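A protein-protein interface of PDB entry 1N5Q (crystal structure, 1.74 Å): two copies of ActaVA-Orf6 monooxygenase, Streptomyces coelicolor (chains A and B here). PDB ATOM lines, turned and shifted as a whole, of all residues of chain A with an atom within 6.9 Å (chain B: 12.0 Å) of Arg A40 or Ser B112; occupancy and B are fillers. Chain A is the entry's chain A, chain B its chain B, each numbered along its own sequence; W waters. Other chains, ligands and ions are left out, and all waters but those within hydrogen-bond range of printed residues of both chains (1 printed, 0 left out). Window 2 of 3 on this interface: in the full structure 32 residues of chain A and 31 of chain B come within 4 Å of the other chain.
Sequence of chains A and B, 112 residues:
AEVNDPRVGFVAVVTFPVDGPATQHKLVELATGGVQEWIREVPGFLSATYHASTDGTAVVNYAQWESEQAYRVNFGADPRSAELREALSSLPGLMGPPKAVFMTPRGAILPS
The backbone carbonyl oxygen of Leu B110 is in hydrogen-bond range of the guanidinium group of Arg A40 (3.1 Å).
NE of Arg A40 is in salt-bridge range of OE1 of Glu A37, 3.1 Å away.
Among the printed residues, pairs that only touch across the chains: Gln A36 with Ile B109, Ile A39 with Ile B109, Arg A40 with Ile B109, Arg A40 with Pro B111, Arg A40 with Ser B112, Phe A45 with Ile B109 and Phe A45 with Pro B111.
Printed residues of chain B within 4 Å of Gln A36: Ile B109 (3.1 Å). No residue of chain B comes within 4 Å of Trp A38. Ile A39 touches one residue of chain B. Of the printed residues of chain B, Arg A40 touches Ile B109 (3.7 Å), Leu B110 (3.1 Å), Pro B111 (3.5 Å) and Ser B112 (3.6 Å). No residue of chain B comes within 4 Å of Glu A41. No residue of chain B comes within 4 Å of Val A42. Phe A45 touches just these residues of chain B: Ile B109 (3.3 Å) and Pro B111 (3.7 Å). Of the printed residues of chain A, Ile B109 touches Gln A36, Ile A39, Arg A40 and Phe A45. Of the printed residues of chain A, Leu B110 touches Arg A40 (3.1 Å). Of the printed residues of chain A, Pro B111 touches Arg A40 (3.5 Å) and Phe A45 (3.7 Å). Of the printed residues of chain A, Ser B112 touches Arg A40 (3.6 Å). The nearest printed residue of chain B that does not touch Arg A40 is Ala B108 (6.7 Å). The nearest printed residue of chain A that does not touch Ser B112 is Glu A41 (6.5 Å). The nearest printed residue of chain A that does not touch Leu B110 is Phe A45 (4.3 Å).
Hydrophobic or aromatic side chains of chain A within 4 Å of the printed part of chain B: Ile A39 and Phe A45. Of the 9 printed residues of chain B, 4 touch a printed residue of chain A. Printed residues of chain B that touch a printed residue of chain A: Ile B109, Leu B110, Pro B111 and Ser B112. Among the printed residues, 8 pairs touch across the chains. Among the printed residues, no Asp or Glu carboxylate lies within 4 Å of a Lys or Arg side-chain nitrogen of the other chain.
No position is printed for both chains.
Water W1 lies within hydrogen-bond range of N of Ser B112 (2.7 Å) and O of Arg A40 (3.3 Å).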
ATOM      1  N   GLN A  36     -11.950  23.536 -13.466  1.00  0.00           N
ATOM      2  CA  GLN A  36     -11.710  24.884 -13.938  1.00  0.00           C
ATOM      3  C   GLN A  36     -12.541  25.274 -15.151  1.00  0.00           C
ATOM      4  O   GLN A  36     -12.174  26.162 -15.884  1.00  0.00           O
ATOM      5  CB  GLN A  36     -10.211  25.143 -14.109  1.00  0.00           C
ATOM      6  CG  GLN A  36      -9.525  24.351 -15.187  1.00  0.00           C
ATOM      7  CD  GLN A  36      -8.022  24.653 -15.136  1.00  0.00           C
ATOM      8  OE1 GLN A  36      -7.616  25.808 -15.181  1.00  0.00           O
ATOM      9  NE2 GLN A  36      -7.191  23.631 -15.001  1.00  0.00           N
ATOM     10  N   GLU A  37     -13.755  24.730 -15.285  1.00  0.00           N
ATOM     11  CA  GLU A  37     -14.641  25.209 -16.345  1.00  0.00           C
ATOM     12  C   GLU A  37     -14.818  26.726 -16.349  1.00  0.00           C
ATOM     13  O   GLU A  37     -14.943  27.395 -17.371  1.00  0.00           O
ATOM     14  CB  GLU A  37     -16.038  24.583 -16.129  1.00  0.00           C
ATOM     15  CG  GLU A  37     -16.066  23.125 -16.548  1.00  0.00           C
ATOM     16  CD  GLU A  37     -15.783  22.920 -18.033  1.00  0.00           C
ATOM     17  OE1 GLU A  37     -16.319  23.696 -18.858  1.00  0.00           O
ATOM     18  OE2 GLU A  37     -14.985  21.995 -18.315  1.00  0.00           O
ATOM     19  N   TRP A  38     -14.885  27.319 -15.143  1.00  0.00           N
ATOM     20  CA  TRP A  38     -15.068  28.764 -15.028  1.00  0.00           C
ATOM     21  C   TRP A  38     -14.005  29.587 -15.730  1.00  0.00           C
ATOM     22  O   TRP A  38     -14.333  30.723 -16.147  1.00  0.00           O
ATOM     23  CB  TRP A  38     -15.121  29.234 -13.573  1.00  0.00           C
ATOM     24  CG  TRP A  38     -13.851  29.012 -12.797  1.00  0.00           C
ATOM     25  CD1 TRP A  38     -13.489  27.854 -12.189  1.00  0.00           C
ATOM     26  CD2 TRP A  38     -12.819  29.958 -12.552  1.00  0.00           C
ATOM     27  NE1 TRP A  38     -12.279  28.002 -11.568  1.00  0.00           N
ATOM     28  CE2 TRP A  38     -11.834  29.282 -11.780  1.00  0.00           C
ATOM     29  CE3 TRP A  38     -12.620  31.294 -12.902  1.00  0.00           C
ATOM     30  CZ2 TRP A  38     -10.683  29.932 -11.363  1.00  0.00           C
ATOM     31  CZ3 TRP A  38     -11.477  31.952 -12.463  1.00  0.00           C
ATOM     32  CH2 TRP A  38     -10.525  31.238 -11.705  1.00  0.00           C
ATOM     33  N   ILE A  39     -12.763  29.113 -15.782  1.00  0.00           N
ATOM     34  CA  ILE A  39     -11.681  29.885 -16.407  1.00  0.00           C
ATOM     35  C   ILE A  39     -11.927  30.164 -17.884  1.00  0.00           C
ATOM     36  O   ILE A  39     -11.467  31.196 -18.412  1.00  0.00           O
ATOM     37  CB  ILE A  39     -10.323  29.162 -16.268  1.00  0.00           C
ATOM     38  CG1 ILE A  39      -9.167  30.181 -16.270  1.00  0.00           C
ATOM     39  CG2 ILE A  39     -10.100  28.072 -17.290  1.00  0.00           C
ATOM     40  CD1 ILE A  39      -7.775  29.553 -16.099  1.00  0.00           C
ATOM     41  N   ARG A  40     -12.689  29.307 -18.594  1.00  0.00           N
ATOM     42  CA  ARG A  40     -12.854  29.481 -20.016  1.00  0.00           C
ATOM     43  C   ARG A  40     -13.537  30.801 -20.386  1.00  0.00           C
ATOM     44  O   ARG A  40     -13.136  31.321 -21.434  1.00  0.00           O
ATOM     45  CB  ARG A  40     -13.549  28.300 -20.705  1.00  0.00           C
ATOM     46  CG  ARG A  40     -12.913  27.021 -20.135  1.00  0.00           C
ATOM     47  CD  ARG A  40     -13.184  25.686 -20.771  1.00  0.00           C
ATOM     48  NE  ARG A  40     -14.613  25.417 -20.849  1.00  0.00           N
ATOM     49  CZ  ARG A  40     -15.345  25.837 -21.884  1.00  0.00           C
ATOM     50  NH1 ARG A  40     -14.774  26.501 -22.881  1.00  0.00           N
ATOM     51  NH2 ARG A  40     -16.640  25.595 -21.865  1.00  0.00           N
ATOM     52  N   GLU A  41     -14.382  31.316 -19.527  1.00  0.00           N
ATOM     53  CA  GLU A  41     -15.076  32.558 -19.851  1.00  0.00           C
ATOM     54  C   GLU A  41     -14.404  33.774 -19.228  1.00  0.00           C
ATOM     55  O   GLU A  41     -14.952  34.861 -19.340  1.00  0.00           O
ATOM     56  CB  GLU A  41     -16.549  32.515 -19.426  1.00  0.00           C
ATOM     57  CG  GLU A  41     -16.797  32.533 -17.940  1.00  0.00           C
ATOM     58  CD  GLU A  41     -18.216  32.300 -17.476  1.00  0.00           C
ATOM     59  OE1 GLU A  41     -19.093  31.865 -18.259  1.00  0.00           O
ATOM     60  OE2 GLU A  41     -18.489  32.536 -16.278  1.00  0.00           O
ATOM     61  N   VAL A  42     -13.219  33.637 -18.654  1.00  0.00           N
ATOM     62  CA  VAL A  42     -12.552  34.787 -18.040  1.00  0.00           C
ATOM     63  C   VAL A  42     -11.958  35.647 -19.134  1.00  0.00           C
ATOM     64  O   VAL A  42     -11.179  35.184 -19.987  1.00  0.00           O
ATOM     65  CB  VAL A  42     -11.433  34.218 -17.121  1.00  0.00           C
ATOM     66  CG1 VAL A  42     -10.494  35.309 -16.649  1.00  0.00           C
ATOM     67  CG2 VAL A  42     -12.004  33.455 -15.927  1.00  0.00           C
ATOM     68  N   PRO A  43     -12.237  36.960 -19.164  1.00  0.00           N
ATOM     69  CA  PRO A  43     -11.656  37.845 -20.139  1.00  0.00           C
ATOM     70  C   PRO A  43     -10.140  37.849 -20.078  1.00  0.00           C
ATOM     71  O   PRO A  43      -9.488  38.005 -19.015  1.00  0.00           O
ATOM     72  CB  PRO A  43     -12.207  39.247 -19.824  1.00  0.00           C
ATOM     73  CG  PRO A  43     -13.313  39.029 -18.855  1.00  0.00           C
ATOM     74  CD  PRO A  43     -13.125  37.672 -18.202  1.00  0.00           C
ATOM     75  N   PHE A  45      -8.299  35.307 -20.880  1.00  0.00           N
ATOM     76  CA  PHE A  45      -7.741  33.923 -20.830  1.00  0.00           C
ATOM     77  C   PHE A  45      -7.645  33.395 -22.247  1.00  0.00           C
ATOM     78  O   PHE A  45      -8.698  33.369 -22.949  1.00  0.00           O
ATOM     79  CB  PHE A  45      -8.670  33.020 -20.006  1.00  0.00           C
ATOM     80  CG  PHE A  45      -8.227  31.567 -20.071  1.00  0.00           C
ATOM     81  CD1 PHE A  45      -7.033  31.173 -19.517  1.00  0.00           C
ATOM     82  CD2 PHE A  45      -9.028  30.627 -20.740  1.00  0.00           C
ATOM     83  CE1 PHE A  45      -6.659  29.810 -19.615  1.00  0.00           C
ATOM     84  CE2 PHE A  45      -8.654  29.314 -20.821  1.00  0.00           C
ATOM     85  CZ  PHE A  45      -7.453  28.896 -20.255  1.00  0.00           C
ATOM     86  N   GLU B   2      -1.483  25.945 -33.229  1.00  0.00           N
ATOM     87  CA  GLU B   2      -2.360  26.218 -32.074  1.00  0.00           C
ATOM     88  C   GLU B   2      -1.849  25.313 -30.947  1.00  0.00           C
ATOM     89  O   GLU B   2      -1.345  24.214 -31.226  1.00  0.00           O
ATOM     90  CB  GLU B   2      -3.774  25.823 -32.488  1.00  0.00           C
ATOM     91  CG  GLU B   2      -4.867  25.968 -31.480  1.00  0.00           C
ATOM     92  CD  GLU B   2      -4.934  27.329 -30.801  1.00  0.00           C
ATOM     93  OE1 GLU B   2      -5.281  28.319 -31.496  1.00  0.00           O
ATOM     94  OE2 GLU B   2      -4.655  27.331 -29.594  1.00  0.00           O
ATOM     95  N   VAL B   3      -1.998  25.733 -29.677  1.00  0.00           N
ATOM     96  CA  VAL B   3      -1.392  24.946 -28.606  1.00  0.00           C
ATOM     97  C   VAL B   3      -1.921  23.532 -28.515  1.00  0.00           C
ATOM     98  O   VAL B   3      -1.202  22.629 -28.024  1.00  0.00           O
ATOM     99  CB  VAL B   3      -1.483  25.615 -27.211  1.00  0.00           C
ATOM    100  CG1 VAL B   3      -0.550  26.841 -27.254  1.00  0.00           C
ATOM    101  CG2 VAL B   3      -2.871  25.987 -26.781  1.00  0.00           C
ATOM    102  N   ASN B   4      -3.194  23.354 -28.890  1.00  0.00           N
ATOM    103  CA  ASN B   4      -3.794  22.022 -28.814  1.00  0.00           C
ATOM    104  C   ASN B   4      -3.961  21.378 -30.182  1.00  0.00           C
ATOM    105  O   ASN B   4      -4.794  20.470 -30.354  1.00  0.00           O
ATOM    106  CB  ASN B   4      -5.182  22.099 -28.130  1.00  0.00           C
ATOM    107  CG  ASN B   4      -6.126  22.900 -29.004  1.00  0.00           C
ATOM    108  OD1 ASN B   4      -5.719  23.914 -29.584  1.00  0.00           O
ATOM    109  ND2 ASN B   4      -7.365  22.424 -29.074  1.00  0.00           N
ATOM    110  N   GLY B 107      -3.413  17.559 -22.341  1.00  0.00           N
ATOM    111  CA  GLY B 107      -4.789  18.100 -22.163  1.00  0.00           C
ATOM    112  C   GLY B 107      -4.717  19.601 -22.218  1.00  0.00           C
ATOM    113  O   GLY B 107      -3.645  20.212 -22.002  1.00  0.00           O
ATOM    114  N   ALA B 108      -5.847  20.224 -22.590  1.00  0.00           N
ATOM    115  CA  ALA B 108      -5.761  21.696 -22.674  1.00  0.00           C
ATOM    116  C   ALA B 108      -7.122  22.304 -22.346  1.00  0.00           C
ATOM    117  O   ALA B 108      -8.169  21.749 -22.722  1.00  0.00           O
ATOM    118  CB  ALA B 108      -5.382  22.205 -24.052  1.00  0.00           C
ATOM    119  N   ILE B 109      -7.077  23.469 -21.743  1.00  0.00           N
ATOM    120  CA  ILE B 109      -8.317  24.204 -21.440  1.00  0.00           C
ATOM    121  C   ILE B 109      -8.329  25.452 -22.298  1.00  0.00           C
ATOM    122  O   ILE B 109      -7.401  26.257 -22.266  1.00  0.00           O
ATOM    123  CB  ILE B 109      -8.344  24.618 -19.985  1.00  0.00           C
ATOM    124  CG1 ILE B 109      -8.397  23.329 -19.145  1.00  0.00           C
ATOM    125  CG2 ILE B 109      -9.540  25.508 -19.630  1.00  0.00           C
ATOM    126  CD1 ILE B 109      -7.314  23.346 -18.116  1.00  0.00           C
ATOM    127  N   LEU B 110      -9.369  25.519 -23.150  1.00  0.00           N
ATOM    128  CA  LEU B 110      -9.448  26.649 -24.081  1.00  0.00           C
ATOM    129  C   LEU B 110     -10.825  27.315 -23.996  1.00  0.00           C
ATOM    130  O   LEU B 110     -11.741  26.602 -23.722  1.00  0.00           O
ATOM    131  CB  LEU B 110      -9.428  26.186 -25.557  1.00  0.00           C
ATOM    132  CG  LEU B 110      -8.072  25.564 -25.924  1.00  0.00           C
ATOM    133  CD1 LEU B 110      -8.349  24.397 -26.849  1.00  0.00           C
ATOM    134  CD2 LEU B 110      -7.163  26.658 -26.425  1.00  0.00           C
ATOM    135  N   PRO B 111     -10.899  28.574 -24.406  1.00  0.00           N
ATOM    136  CA  PRO B 111     -12.167  29.265 -24.470  1.00  0.00           C
ATOM    137  C   PRO B 111     -12.989  28.757 -25.637  1.00  0.00           C
ATOM    138  O   PRO B 111     -12.438  28.175 -26.591  1.00  0.00           O
ATOM    139  CB  PRO B 111     -11.747  30.717 -24.629  1.00  0.00           C
ATOM    140  CG  PRO B 111     -10.325  30.766 -25.017  1.00  0.00           C
ATOM    141  CD  PRO B 111      -9.732  29.394 -24.821  1.00  0.00           C
ATOM    142  N   SER B 112     -14.315  28.858 -25.513  1.00  0.00           N
ATOM    143  CA  SER B 112     -15.185  28.362 -26.581  1.00  0.00           C
ATOM    144  C   SER B 112     -15.553  29.525 -27.519  1.00  0.00           C
ATOM    145  O   SER B 112     -14.758  30.512 -27.468  1.00  0.00           O
ATOM    146  CB  SER B 112     -16.479  27.751 -26.046  1.00  0.00           C
ATOM    147  OG  SER B 112     -17.545  28.679 -26.186  1.00  0.00           O
ATOM    148  OXT SER B 112     -15.995  29.172 -28.645  1.00  0.00           O
HETATM  149  O   HOH W   1     -15.521  30.230 -23.476  1.00  0.00           O
